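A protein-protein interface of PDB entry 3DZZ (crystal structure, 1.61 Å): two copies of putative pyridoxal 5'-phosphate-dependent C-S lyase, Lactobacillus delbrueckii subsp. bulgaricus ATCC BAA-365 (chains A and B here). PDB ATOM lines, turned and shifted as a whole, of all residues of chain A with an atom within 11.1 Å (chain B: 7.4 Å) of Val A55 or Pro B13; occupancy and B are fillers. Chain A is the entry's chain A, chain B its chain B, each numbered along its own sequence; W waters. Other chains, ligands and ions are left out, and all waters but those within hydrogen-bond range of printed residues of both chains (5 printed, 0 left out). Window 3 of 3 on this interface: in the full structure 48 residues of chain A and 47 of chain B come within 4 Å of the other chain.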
ATOM      1  N   ALA A  47      -2.949 -20.878 -11.789  1.00  0.00           N
ATOM      2  CA  ALA A  47      -4.301 -20.346 -11.583  1.00  0.00           C
ATOM      3  C   ALA A  47      -5.208 -20.766 -12.739  1.00  0.00           C
ATOM      4  O   ALA A  47      -6.378 -21.055 -12.528  1.00  0.00           O
ATOM      5  CB  ALA A  47      -4.313 -18.850 -11.423  1.00  0.00           C
ATOM      6  N   SER A  48      -4.680 -20.696 -13.955  1.00  0.00           N
ATOM      7  CA  SER A  48      -5.449 -21.060 -15.151  1.00  0.00           C
ATOM      8  C   SER A  48      -5.786 -22.531 -15.159  1.00  0.00           C
ATOM      9  O   SER A  48      -6.872 -22.936 -15.560  1.00  0.00           O
ATOM     10  CB  SER A  48      -4.742 -20.689 -16.435  1.00  0.00           C
ATOM     11  OG  SER A  48      -3.660 -21.579 -16.693  1.00  0.00           O
ATOM     12  N   MET A  49      -4.851 -23.340 -14.671  1.00  0.00           N
ATOM     13  CA  MET A  49      -5.056 -24.794 -14.626  1.00  0.00           C
ATOM     14  C   MET A  49      -6.127 -25.123 -13.578  1.00  0.00           C
ATOM     15  O   MET A  49      -7.011 -25.992 -13.804  1.00  0.00           O
ATOM     16  CB  MET A  49      -3.784 -25.557 -14.289  1.00  0.00           C
ATOM     17  CG  MET A  49      -2.690 -25.529 -15.278  1.00  0.00           C
ATOM     18  SD  MET A  49      -1.134 -26.426 -14.561  1.00  0.00           S
ATOM     19  CE  MET A  49      -0.035 -26.624 -16.154  1.00  0.00           C
ATOM     20  N   GLU A  50      -6.011 -24.518 -12.384  1.00  0.00           N
ATOM     21  CA  GLU A  50      -7.031 -24.722 -11.355  1.00  0.00           C
ATOM     22  C   GLU A  50      -8.406 -24.331 -11.857  1.00  0.00           C
ATOM     23  O   GLU A  50      -9.383 -25.086 -11.654  1.00  0.00           O
ATOM     24  CB  GLU A  50      -6.665 -23.953 -10.067  1.00  0.00           C
ATOM     25  CG  GLU A  50      -5.496 -24.544  -9.333  1.00  0.00           C
ATOM     26  CD  GLU A  50      -5.861 -25.793  -8.552  1.00  0.00           C
ATOM     27  OE1 GLU A  50      -7.041 -26.218  -8.611  1.00  0.00           O
ATOM     28  OE2 GLU A  50      -4.983 -26.354  -7.847  1.00  0.00           O
ATOM     29  N   GLU A  51      -8.511 -23.214 -12.580  1.00  0.00           N
ATOM     30  CA  GLU A  51      -9.846 -22.746 -13.019  1.00  0.00           C
ATOM     31  C   GLU A  51     -10.447 -23.697 -14.027  1.00  0.00           C
ATOM     32  O   GLU A  51     -11.615 -23.996 -14.018  1.00  0.00           O
ATOM     33  CB  GLU A  51      -9.749 -21.368 -13.656  1.00  0.00           C
ATOM     34  CG  GLU A  51     -11.072 -20.853 -14.231  1.00  0.00           C
ATOM     35  CD  GLU A  51     -10.991 -19.348 -14.501  1.00  0.00           C
ATOM     36  OE1 GLU A  51      -9.862 -18.836 -14.663  1.00  0.00           O
ATOM     37  OE2 GLU A  51     -12.034 -18.680 -14.529  1.00  0.00           O
ATOM     38  N   LYS A  52      -9.583 -24.213 -14.896  1.00  0.00           N
ATOM     39  CA  LYS A  52     -10.024 -25.190 -15.895  1.00  0.00           C
ATOM     40  C   LYS A  52     -10.503 -26.468 -15.254  1.00  0.00           C
ATOM     41  O   LYS A  52     -11.522 -27.024 -15.669  1.00  0.00           O
ATOM     42  CB  LYS A  52      -8.893 -25.474 -16.922  1.00  0.00           C
ATOM     43  CG  LYS A  52      -9.278 -26.517 -17.966  1.00  0.00           C
ATOM     44  CD  LYS A  52     -10.505 -26.177 -18.787  1.00  0.00           C
ATOM     45  CE  LYS A  52     -10.745 -27.118 -19.949  1.00  0.00           C
ATOM     46  NZ  LYS A  52      -9.719 -26.984 -21.068  1.00  0.00           N
ATOM     47  N   LEU A  53      -9.819 -26.941 -14.222  1.00  0.00           N
ATOM     48  CA  LEU A  53     -10.274 -28.157 -13.559  1.00  0.00           C
ATOM     49  C   LEU A  53     -11.677 -28.045 -13.017  1.00  0.00           C
ATOM     50  O   LEU A  53     -12.416 -28.992 -12.975  1.00  0.00           O
ATOM     51  CB  LEU A  53      -9.351 -28.558 -12.443  1.00  0.00           C
ATOM     52  CG  LEU A  53      -8.070 -29.213 -12.925  1.00  0.00           C
ATOM     53  CD1 LEU A  53      -7.511 -29.868 -11.649  1.00  0.00           C
ATOM     54  CD2 LEU A  53      -8.189 -30.215 -14.101  1.00  0.00           C
ATOM     55  N   LYS A  54     -12.032 -26.841 -12.628  1.00  0.00           N
ATOM     56  CA  LYS A  54     -13.338 -26.656 -12.047  1.00  0.00           C
ATOM     57  C   LYS A  54     -14.488 -26.883 -12.998  1.00  0.00           C
ATOM     58  O   LYS A  54     -15.650 -26.987 -12.577  1.00  0.00           O
ATOM     59  CB  LYS A  54     -13.460 -25.294 -11.359  1.00  0.00           C
ATOM     60  CG  LYS A  54     -12.520 -25.013 -10.179  1.00  0.00           C
ATOM     61  CD  LYS A  54     -12.214 -26.200  -9.300  1.00  0.00           C
ATOM     62  CE  LYS A  54     -10.923 -25.976  -8.439  1.00  0.00           C
ATOM     63  NZ  LYS A  54      -9.561 -26.387  -9.087  1.00  0.00           N
ATOM     64  N   VAL A  55     -14.227 -26.919 -14.283  1.00  0.00           N
ATOM     65  CA  VAL A  55     -15.273 -27.277 -15.226  1.00  0.00           C
ATOM     66  C   VAL A  55     -15.872 -28.672 -14.866  1.00  0.00           C
ATOM     67  O   VAL A  55     -17.074 -28.887 -14.901  1.00  0.00           O
ATOM     68  CB  VAL A  55     -14.778 -27.277 -16.668  1.00  0.00           C
ATOM     69  CG1 VAL A  55     -15.833 -27.897 -17.646  1.00  0.00           C
ATOM     70  CG2 VAL A  55     -14.303 -25.845 -17.119  1.00  0.00           C
ATOM     71  N   ALA A  56     -15.008 -29.553 -14.421  1.00  0.00           N
ATOM     72  CA  ALA A  56     -15.379 -30.875 -13.921  1.00  0.00           C
ATOM     73  C   ALA A  56     -16.022 -31.785 -14.965  1.00  0.00           C
ATOM     74  O   ALA A  56     -16.836 -32.658 -14.668  1.00  0.00           O
ATOM     75  CB  ALA A  56     -16.260 -30.760 -12.672  1.00  0.00           C
ATOM     76  N   ALA A  57     -15.623 -31.572 -16.207  1.00  0.00           N
ATOM     77  CA  ALA A  57     -16.067 -32.353 -17.383  1.00  0.00           C
ATOM     78  C   ALA A  57     -15.084 -32.052 -18.478  1.00  0.00           C
ATOM     79  O   ALA A  57     -14.785 -30.872 -18.675  1.00  0.00           O
ATOM     80  CB  ALA A  57     -17.478 -31.979 -17.823  1.00  0.00           C
ATOM     81  N   PHE A  58     -14.503 -33.078 -19.119  1.00  0.00           N
ATOM     82  CA  PHE A  58     -13.374 -32.847 -19.978  1.00  0.00           C
ATOM     83  C   PHE A  58     -13.616 -33.493 -21.366  1.00  0.00           C
ATOM     84  O   PHE A  58     -12.917 -34.402 -21.814  1.00  0.00           O
ATOM     85  CB  PHE A  58     -12.079 -33.275 -19.245  1.00  0.00           C
ATOM     86  CG  PHE A  58     -11.916 -32.531 -17.954  1.00  0.00           C
ATOM     87  CD1 PHE A  58     -11.733 -31.153 -17.979  1.00  0.00           C
ATOM     88  CD2 PHE A  58     -12.020 -33.178 -16.730  1.00  0.00           C
ATOM     89  CE1 PHE A  58     -11.698 -30.425 -16.799  1.00  0.00           C
ATOM     90  CE2 PHE A  58     -11.956 -32.445 -15.550  1.00  0.00           C
ATOM     91  CZ  PHE A  58     -11.743 -31.062 -15.601  1.00  0.00           C
ATOM     92  N   GLY A  59     -14.602 -32.964 -22.048  1.00  0.00           N
ATOM     93  CA  GLY A  59     -14.861 -33.376 -23.418  1.00  0.00           C
ATOM     94  C   GLY A  59     -13.962 -32.728 -24.448  1.00  0.00           C
ATOM     95  O   GLY A  59     -12.940 -32.130 -24.133  1.00  0.00           O
ATOM     96  N   TYR A  60     -14.357 -32.889 -25.689  1.00  0.00           N
ATOM     97  CA  TYR A  60     -13.510 -32.448 -26.802  1.00  0.00           C
ATOM     98  C   TYR A  60     -13.380 -30.929 -26.875  1.00  0.00           C
ATOM     99  O   TYR A  60     -14.342 -30.143 -26.660  1.00  0.00           O
ATOM    100  CB  TYR A  60     -14.074 -32.978 -28.117  1.00  0.00           C
ATOM    101  CG  TYR A  60     -14.113 -34.468 -28.187  1.00  0.00           C
ATOM    102  CD1 TYR A  60     -12.978 -35.176 -28.465  1.00  0.00           C
ATOM    103  CD2 TYR A  60     -15.288 -35.167 -27.888  1.00  0.00           C
ATOM    104  CE1 TYR A  60     -13.004 -36.591 -28.520  1.00  0.00           C
ATOM    105  CE2 TYR A  60     -15.317 -36.570 -27.927  1.00  0.00           C
ATOM    106  CZ  TYR A  60     -14.162 -37.249 -28.241  1.00  0.00           C
ATOM    107  OH  TYR A  60     -14.100 -38.631 -28.301  1.00  0.00           O
ATOM    108  N   GLU A  61     -12.178 -30.510 -27.185  1.00  0.00           N
ATOM    109  CA  GLU A  61     -11.849 -29.086 -27.267  1.00  0.00           C
ATOM    110  C   GLU A  61     -11.273 -28.765 -28.610  1.00  0.00           C
ATOM    111  O   GLU A  61     -10.563 -29.560 -29.194  1.00  0.00           O
ATOM    112  CB  GLU A  61     -10.730 -28.786 -26.279  1.00  0.00           C
ATOM    113  CG  GLU A  61     -11.225 -28.833 -24.914  1.00  0.00           C
ATOM    114  CD  GLU A  61     -10.245 -28.317 -23.891  1.00  0.00           C
ATOM    115  OE1 GLU A  61      -9.435 -27.345 -24.160  1.00  0.00           O
ATOM    116  OE2 GLU A  61     -10.338 -28.876 -22.793  1.00  0.00           O
ATOM    117  N   ASN A 270      -5.100 -31.637 -25.148  1.00  0.00           N
ATOM    118  CA  ASN A 270      -5.606 -32.201 -23.905  1.00  0.00           C
ATOM    119  C   ASN A 270      -6.302 -31.113 -23.070  1.00  0.00           C
ATOM    120  O   ASN A 270      -6.332 -29.939 -23.453  1.00  0.00           O
ATOM    121  CB  ASN A 270      -4.501 -32.962 -23.122  1.00  0.00           C
ATOM    122  CG  ASN A 270      -3.468 -32.058 -22.546  1.00  0.00           C
ATOM    123  OD1 ASN A 270      -3.797 -30.997 -21.999  1.00  0.00           O
ATOM    124  ND2 ASN A 270      -2.191 -32.430 -22.719  1.00  0.00           N
ATOM    125  N   LEU A 271      -6.851 -31.543 -21.932  1.00  0.00           N
ATOM    126  CA  LEU A 271      -7.711 -30.698 -21.066  1.00  0.00           C
ATOM    127  C   LEU A 271      -7.036 -29.460 -20.443  1.00  0.00           C
ATOM    128  O   LEU A 271      -7.749 -28.568 -20.022  1.00  0.00           O
ATOM    129  CB  LEU A 271      -8.348 -31.513 -19.928  1.00  0.00           C
ATOM    130  CG  LEU A 271      -7.474 -32.061 -18.797  1.00  0.00           C
ATOM    131  CD1 LEU A 271      -8.231 -33.106 -18.057  1.00  0.00           C
ATOM    132  CD2 LEU A 271      -6.151 -32.715 -19.247  1.00  0.00           C
ATOM    133  N   LEU A 272      -5.708 -29.384 -20.467  1.00  0.00           N
ATOM    134  CA  LEU A 272      -5.004 -28.230 -19.916  1.00  0.00           C
ATOM    135  C   LEU A 272      -4.200 -27.436 -20.916  1.00  0.00           C
ATOM    136  O   LEU A 272      -3.837 -26.290 -20.614  1.00  0.00           O
ATOM    137  CB  LEU A 272      -4.121 -28.575 -18.721  1.00  0.00           C
ATOM    138  CG  LEU A 272      -4.808 -29.086 -17.437  1.00  0.00           C
ATOM    139  CD1 LEU A 272      -3.794 -29.433 -16.321  1.00  0.00           C
ATOM    140  CD2 LEU A 272      -5.861 -28.111 -16.874  1.00  0.00           C
ATOM    141  N   PRO A 275      -5.716 -23.546 -21.911  1.00  0.00           N
ATOM    142  CA  PRO A 275      -5.626 -22.486 -20.911  1.00  0.00           C
ATOM    143  C   PRO A 275      -4.240 -22.259 -20.326  1.00  0.00           C
ATOM    144  O   PRO A 275      -3.867 -21.109 -20.021  1.00  0.00           O
ATOM    145  CB  PRO A 275      -6.659 -22.917 -19.851  1.00  0.00           C
ATOM    146  CG  PRO A 275      -6.857 -24.375 -20.096  1.00  0.00           C
ATOM    147  CD  PRO A 275      -6.698 -24.592 -21.534  1.00  0.00           C
ATOM    148  N   ASP B   8     -23.783 -36.335  -8.571  1.00  0.00           N
ATOM    149  CA  ASP B   8     -24.617 -35.319  -9.240  1.00  0.00           C
ATOM    150  C   ASP B   8     -24.834 -35.652 -10.724  1.00  0.00           C
ATOM    151  O   ASP B   8     -23.872 -35.589 -11.498  1.00  0.00           O
ATOM    152  CB  ASP B   8     -23.917 -33.963  -9.125  1.00  0.00           C
ATOM    153  CG  ASP B   8     -24.699 -32.800  -9.756  1.00  0.00           C
ATOM    154  OD1 ASP B   8     -25.554 -33.000 -10.639  1.00  0.00           O
ATOM    155  OD2 ASP B   8     -24.409 -31.643  -9.374  1.00  0.00           O
ATOM    156  N   THR B  10     -27.531 -34.144 -12.317  1.00  0.00           N
ATOM    157  CA  THR B  10     -28.575 -33.166 -12.611  1.00  0.00           C
ATOM    158  C   THR B  10     -28.082 -31.802 -13.089  1.00  0.00           C
ATOM    159  O   THR B  10     -28.850 -31.075 -13.728  1.00  0.00           O
ATOM    160  CB  THR B  10     -29.540 -33.013 -11.399  1.00  0.00           C
ATOM    161  OG1 THR B  10     -28.922 -32.239 -10.359  1.00  0.00           O
ATOM    162  CG2 THR B  10     -29.929 -34.394 -10.856  1.00  0.00           C
ATOM    163  N   HIS B  11     -26.842 -31.434 -12.759  1.00  0.00           N
ATOM    164  CA  HIS B  11     -26.255 -30.171 -13.241  1.00  0.00           C
ATOM    165  C   HIS B  11     -25.297 -30.386 -14.370  1.00  0.00           C
ATOM    166  O   HIS B  11     -24.413 -31.247 -14.283  1.00  0.00           O
ATOM    167  CB  HIS B  11     -25.532 -29.415 -12.133  1.00  0.00           C
ATOM    168  CG  HIS B  11     -26.430 -29.112 -10.979  1.00  0.00           C
ATOM    169  ND1 HIS B  11     -26.540 -29.944  -9.886  1.00  0.00           N
ATOM    170  CD2 HIS B  11     -27.310 -28.105 -10.778  1.00  0.00           C
ATOM    171  CE1 HIS B  11     -27.426 -29.443  -9.045  1.00  0.00           C
ATOM    172  NE2 HIS B  11     -27.907 -28.327  -9.562  1.00  0.00           N
ATOM    173  N   VAL B  12     -25.544 -29.646 -15.444  1.00  0.00           N
ATOM    174  CA  VAL B  12     -24.670 -29.669 -16.616  1.00  0.00           C
ATOM    175  C   VAL B  12     -23.409 -28.842 -16.335  1.00  0.00           C
ATOM    176  O   VAL B  12     -23.459 -27.645 -15.955  1.00  0.00           O
ATOM    177  CB  VAL B  12     -25.369 -29.061 -17.877  1.00  0.00           C
ATOM    178  CG1 VAL B  12     -24.461 -29.055 -19.082  1.00  0.00           C
ATOM    179  CG2 VAL B  12     -26.677 -29.807 -18.214  1.00  0.00           C
ATOM    180  N   PRO B  13     -22.253 -29.455 -16.532  1.00  0.00           N
ATOM    181  CA  PRO B  13     -21.021 -28.722 -16.351  1.00  0.00           C
ATOM    182  C   PRO B  13     -20.959 -27.466 -17.222  1.00  0.00           C
ATOM    183  O   PRO B  13     -21.243 -27.535 -18.424  1.00  0.00           O
ATOM    184  CB  PRO B  13     -19.959 -29.735 -16.797  1.00  0.00           C
ATOM    185  CG  PRO B  13     -20.596 -31.066 -16.556  1.00  0.00           C
ATOM    186  CD  PRO B  13     -22.054 -30.866 -16.819  1.00  0.00           C
ATOM    187  N   LYS B  14     -20.460 -26.381 -16.653  1.00  0.00           N
ATOM    188  CA  LYS B  14     -20.310 -25.133 -17.387  1.00  0.00           C
ATOM    189  C   LYS B  14     -18.939 -25.095 -18.053  1.00  0.00           C
ATOM    190  O   LYS B  14     -17.911 -24.996 -17.400  1.00  0.00           O
ATOM    191  CB  LYS B  14     -20.487 -23.931 -16.484  1.00  0.00           C
ATOM    192  N   ARG B  15     -18.937 -25.222 -19.364  1.00  0.00           N
ATOM    193  CA  ARG B  15     -17.704 -25.331 -20.126  1.00  0.00           C
ATOM    194  C   ARG B  15     -17.046 -23.968 -20.417  1.00  0.00           C
ATOM    195  O   ARG B  15     -17.689 -22.919 -20.454  1.00  0.00           O
ATOM    196  CB  ARG B  15     -17.921 -26.035 -21.467  1.00  0.00           C
ATOM    197  CG  ARG B  15     -18.681 -27.372 -21.517  1.00  0.00           C
ATOM    198  CD  ARG B  15     -18.458 -28.359 -20.460  1.00  0.00           C
ATOM    199  NE  ARG B  15     -18.693 -29.697 -21.020  1.00  0.00           N
ATOM    200  CZ  ARG B  15     -19.826 -30.398 -20.948  1.00  0.00           C
ATOM    201  NH1 ARG B  15     -20.908 -29.956 -20.301  1.00  0.00           N
ATOM    202  NH2 ARG B  15     -19.858 -31.567 -21.530  1.00  0.00           N
ATOM    203  N   GLN B  16     -15.759 -24.024 -20.689  1.00  0.00           N
ATOM    204  CA  GLN B  16     -15.039 -22.907 -21.282  1.00  0.00           C
ATOM    205  C   GLN B  16     -15.388 -22.774 -22.766  1.00  0.00           C
ATOM    206  O   GLN B  16     -16.015 -23.612 -23.370  1.00  0.00           O
ATOM    207  CB  GLN B  16     -13.523 -23.002 -21.093  1.00  0.00           C
ATOM    208  CG  GLN B  16     -13.176 -23.028 -19.583  1.00  0.00           C
ATOM    209  CD  GLN B  16     -11.757 -22.729 -19.280  1.00  0.00           C
ATOM    210  OE1 GLN B  16     -10.910 -22.732 -20.154  1.00  0.00           O
ATOM    211  NE2 GLN B  16     -11.483 -22.456 -18.001  1.00  0.00           N
ATOM    212  N   TRP B  22     -20.414 -27.502 -26.761  1.00  0.00           N
ATOM    213  CA  TRP B  22     -21.194 -26.348 -26.265  1.00  0.00           C
ATOM    214  C   TRP B  22     -20.701 -25.017 -26.741  1.00  0.00           C
ATOM    215  O   TRP B  22     -21.194 -23.994 -26.308  1.00  0.00           O
ATOM    216  CB  TRP B  22     -21.188 -26.314 -24.735  1.00  0.00           C
ATOM    217  CG  TRP B  22     -22.045 -27.370 -24.160  1.00  0.00           C
ATOM    218  CD1 TRP B  22     -21.667 -28.609 -23.729  1.00  0.00           C
ATOM    219  CD2 TRP B  22     -23.463 -27.298 -23.975  1.00  0.00           C
ATOM    220  NE1 TRP B  22     -22.761 -29.316 -23.296  1.00  0.00           N
ATOM    221  CE2 TRP B  22     -23.873 -28.529 -23.404  1.00  0.00           C
ATOM    222  CE3 TRP B  22     -24.422 -26.321 -24.251  1.00  0.00           C
ATOM    223  CZ2 TRP B  22     -25.192 -28.809 -23.095  1.00  0.00           C
ATOM    224  CZ3 TRP B  22     -25.721 -26.585 -23.927  1.00  0.00           C
ATOM    225  CH2 TRP B  22     -26.105 -27.827 -23.351  1.00  0.00           C
ATOM    226  N   MET B  37     -20.358 -36.510 -22.259  1.00  0.00           N
ATOM    227  CA  MET B  37     -21.500 -36.384 -21.378  1.00  0.00           C
ATOM    228  C   MET B  37     -21.700 -35.009 -20.869  1.00  0.00           C
ATOM    229  O   MET B  37     -20.740 -34.221 -20.716  1.00  0.00           O
ATOM    230  CB  MET B  37     -21.269 -37.256 -20.188  1.00  0.00           C
ATOM    231  CG  MET B  37     -21.011 -38.687 -20.542  1.00  0.00           C
ATOM    232  SD  MET B  37     -20.852 -39.735 -18.903  1.00  0.00           S
ATOM    233  CE  MET B  37     -20.105 -41.412 -19.488  1.00  0.00           C
ATOM    234  N   ASP B  38     -22.937 -34.755 -20.453  1.00  0.00           N
ATOM    235  CA  ASP B  38     -23.253 -33.525 -19.690  1.00  0.00           C
ATOM    236  C   ASP B  38     -23.411 -33.754 -18.198  1.00  0.00           C
ATOM    237  O   ASP B  38     -24.365 -33.315 -17.558  1.00  0.00           O
ATOM    238  CB  ASP B  38     -24.431 -32.832 -20.320  1.00  0.00           C
ATOM    239  CG  ASP B  38     -24.037 -32.205 -21.618  1.00  0.00           C
ATOM    240  OD1 ASP B  38     -22.961 -31.542 -21.671  1.00  0.00           O
ATOM    241  OD2 ASP B  38     -24.754 -32.400 -22.610  1.00  0.00           O
ATOM    242  N   PHE B  39     -22.462 -34.513 -17.676  1.00  0.00           N
ATOM    243  CA  PHE B  39     -22.410 -34.834 -16.265  1.00  0.00           C
ATOM    244  C   PHE B  39     -21.035 -34.480 -15.783  1.00  0.00           C
ATOM    245  O   PHE B  39     -20.032 -34.662 -16.538  1.00  0.00           O
ATOM    246  CB  PHE B  39     -22.621 -36.346 -16.028  1.00  0.00           C
ATOM    247  CG  PHE B  39     -23.950 -36.883 -16.440  1.00  0.00           C
ATOM    248  CD1 PHE B  39     -25.135 -36.256 -16.048  1.00  0.00           C
ATOM    249  CD2 PHE B  39     -24.020 -38.015 -17.237  1.00  0.00           C
ATOM    250  CE1 PHE B  39     -26.370 -36.808 -16.424  1.00  0.00           C
ATOM    251  CE2 PHE B  39     -25.218 -38.559 -17.590  1.00  0.00           C
ATOM    252  CZ  PHE B  39     -26.414 -37.914 -17.184  1.00  0.00           C
ATOM    253  N   LYS B  40     -20.971 -34.000 -14.539  1.00  0.00           N
ATOM    254  CA  LYS B  40     -19.685 -33.774 -13.923  1.00  0.00           C
ATOM    255  C   LYS B  40     -19.009 -35.116 -13.709  1.00  0.00           C
ATOM    256  O   LYS B  40     -19.637 -36.138 -13.537  1.00  0.00           O
ATOM    257  CB  LYS B  40     -19.868 -33.045 -12.609  1.00  0.00           C
ATOM    258  CG  LYS B  40     -20.366 -31.604 -12.806  1.00  0.00           C
ATOM    259  CD  LYS B  40     -20.640 -30.906 -11.483  1.00  0.00           C
ATOM    260  CE  LYS B  40     -20.865 -29.415 -11.704  1.00  0.00           C
ATOM    261  NZ  LYS B  40     -22.229 -29.059 -12.230  1.00  0.00           N
ATOM    262  N   ILE B  41     -17.693 -35.112 -13.761  1.00  0.00           N
ATOM    263  CA  ILE B  41     -16.951 -36.304 -13.455  1.00  0.00           C
ATOM    264  C   ILE B  41     -16.979 -36.704 -11.967  1.00  0.00           C
ATOM    265  O   ILE B  41     -17.334 -35.903 -11.072  1.00  0.00           O
ATOM    266  CB  ILE B  41     -15.456 -36.193 -13.955  1.00  0.00           C
ATOM    267  CG1 ILE B  41     -14.616 -35.260 -13.116  1.00  0.00           C
ATOM    268  CG2 ILE B  41     -15.382 -35.856 -15.440  1.00  0.00           C
ATOM    269  CD1 ILE B  41     -13.173 -35.292 -13.506  1.00  0.00           C
ATOM    270  N   MET B  46     -11.604 -36.040  -9.812  1.00  0.00           N
ATOM    271  CA  MET B  46     -11.276 -34.619  -9.556  1.00  0.00           C
ATOM    272  C   MET B  46     -10.267 -34.517  -8.440  1.00  0.00           C
ATOM    273  O   MET B  46      -9.300 -33.775  -8.545  1.00  0.00           O
ATOM    274  CB  MET B  46     -12.513 -33.821  -9.145  1.00  0.00           C
ATOM    275  CG  MET B  46     -13.452 -33.447 -10.261  1.00  0.00           C
ATOM    276  SD  MET B  46     -12.675 -31.996 -11.379  1.00  0.00           S
ATOM    277  CE  MET B  46     -11.376 -31.331 -10.264  1.00  0.00           C
ATOM    278  N   ASN B 237     -16.257 -39.417 -18.938  1.00  0.00           N
ATOM    279  CA  ASN B 237     -16.339 -38.097 -19.502  1.00  0.00           C
ATOM    280  C   ASN B 237     -15.000 -37.345 -19.527  1.00  0.00           C
ATOM    281  O   ASN B 237     -14.838 -36.247 -19.055  1.00  0.00           O
ATOM    282  CB  ASN B 237     -17.393 -37.268 -18.778  1.00  0.00           C
ATOM    283  CG  ASN B 237     -17.923 -36.173 -19.664  1.00  0.00           C
ATOM    284  OD1 ASN B 237     -17.743 -36.186 -20.892  1.00  0.00           O
ATOM    285  ND2 ASN B 237     -18.585 -35.168 -19.029  1.00  0.00           N
ATOM    286  N   PRO B 371     -28.506 -34.831 -18.222  1.00  0.00           N
ATOM    287  CA  PRO B 371     -29.579 -34.861 -17.258  1.00  0.00           C
ATOM    288  C   PRO B 371     -30.945 -35.185 -17.874  1.00  0.00           C
ATOM    289  O   PRO B 371     -31.221 -34.811 -19.027  1.00  0.00           O
ATOM    290  CB  PRO B 371     -29.532 -33.456 -16.682  1.00  0.00           C
ATOM    291  CG  PRO B 371     -28.067 -33.112 -16.760  1.00  0.00           C
ATOM    292  CD  PRO B 371     -27.656 -33.636 -18.062  1.00  0.00           C
HETATM  293  O   HOH W   1     -10.153 -24.455 -22.181  1.00  0.00           O
HETATM  294  O   HOH W   2      -8.712 -21.542 -17.033  1.00  0.00           O
HETATM  295  O   HOH W   3     -13.489 -22.850 -15.858  1.00  0.00           O
HETATM  296  O   HOH W   4     -16.102 -30.316 -21.999  1.00  0.00           O
HETATM  297  O   HOH W   5     -19.051 -27.147 -13.961  1.00  0.00           O
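O of Ala A56 lies within hydrogen-bond range of N of Ile B41 (2.8 Å).
The backbone carbonyl oxygen (O) of Asn B237 sits at hydrogen-bond distance from the backbone NH (N) of Phe A58, at 3.2 Å.
The side-chain sulfur (SD) of Met B46 sits close to the backbone carbonyl oxygen (O) of Leu A53, 3.4 Å away.
The side-chain carboxylate of Glu A61 lies within salt-bridge range of the side-chain amino group of Lys A52, 2.6 Å away.
The side-chain amino group (NZ) of Lys A52 lies within hydrogen-bond range of the backbone carbonyl oxygen (O) of Leu A271, 2.7 Å away.
NH2 of Arg B15 is in hydrogen-bond range of O of Met B37, 2.9 Å away.
The side-chain carboxylate of Asp B38 is in salt-bridge range of the guanidinium group of Arg B15, 2.9 Å away.
The backbone carbonyl oxygen (O) of Met B37 lies within hydrogen-bond range of the side-chain amide nitrogen (ND2) of Asn B237.
The backbone carbonyl oxygen of Phe B39 lies within hydrogen-bond range of the side-chain amide nitrogen of Asn B237 (2.9 Å).
CB of Pro B13 touches O of Val A55, at 3.6 Å.
Lys B14 touches Val A55.
Val A55 touches Arg B15 (CG1 to CD, 3.9 Å).
Gln B16 touches Val A55 (CG to CG2, 3.9 Å).
Ala A56 touches Lys B40.
Ala A56 touches Met B46.
CG of Pro B13 touches CB of Ala A57, 3.5 Å away.
Ala A57 touches Phe B39 (CB to O, 3.9 Å).
Asn B237 touches Ala A57.
Phe A58 touches Ile B41.
Of chain B, only Pro B13, Lys B14, Arg B15 and Gln B16 come within 4 Å of Val A55.
Printed residues of chain A within 4 Å of Pro B13: Val A55 (3.6 Å) and Ala A57 (3.5 Å).
No residue of chain A comes within 4 Å of Val B12.
Arg B15 touches just one residue of chain A: Val A55.
Gln B16 touches just these residues of chain A: Lys A52 (3.7 Å) and Val A55 (3.9 Å).
No residue of chain A comes within 4 Å of Asp B38.
Lys B40 touches just one residue of chain A: Ala A56.
Of the printed residues of chain B, Lys A52 touches Gln B16.
Of the printed residues of chain B, Phe A58 touches Ile B41 and Asn B237.
Of the printed residues of chain B, Ala A57 touches Pro B13 (3.5 Å), Phe B39 (3.9 Å) and Asn B237 (3.6 Å).
Printed residues of chain A within 4 Å of Met B46: Leu A53 and Ala A56.
Of the printed residues of chain A, Ile B41 touches Ala A56 (2.8 Å) and Phe A58 (3.7 Å).
The nearest residue of chain B that does not touch Val A55 is Lys B40 (4.8 Å).
The nearest residue of chain A that does not touch Pro B13 is Ala A56 (4.5 Å).
Hydrophobic or aromatic side chains of chain A that line the printed part of chain B: Val A55, Ala A57 and Phe A58.
Printed residues of chain B that touch a printed residue of chain A: Pro B13, Lys B14, Arg B15, Gln B16, Phe B39, Lys B40, Ile B41, Met B46 and Asn B237.
Among the printed residues, no Asp or Glu carboxylate lies within 4 Å of a Lys or Arg side-chain nitrogen of the other chain.
No position is printed for both chains.
Of the 14 pairs that touch across the chains among the printed residues, none has its exchanged pair printed and touching as well.
Water W2 lies within hydrogen-bond range of the backbone carbonyl oxygen (O) of Ser A48 (2.7 Å) and the side-chain amide nitrogen (NE2) of Gln B16 (3.1 Å).
Water W1 bridges OE1 of Gln B16 and NZ of Lys A52.
Water W5 lies within hydrogen-bond range of O of Val A55 and N of Lys B14.
Water W4 lies within hydrogen-bond range of NE of Arg B15 (2.8 Å) and N of Gly A59 (3.0 Å).
Water W3 bridges the backbone carbonyl oxygen (O) of Glu A51 (2.9 Å) and the side-chain amide nitrogen (NE2) of Gln B16 (3.0 Å).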
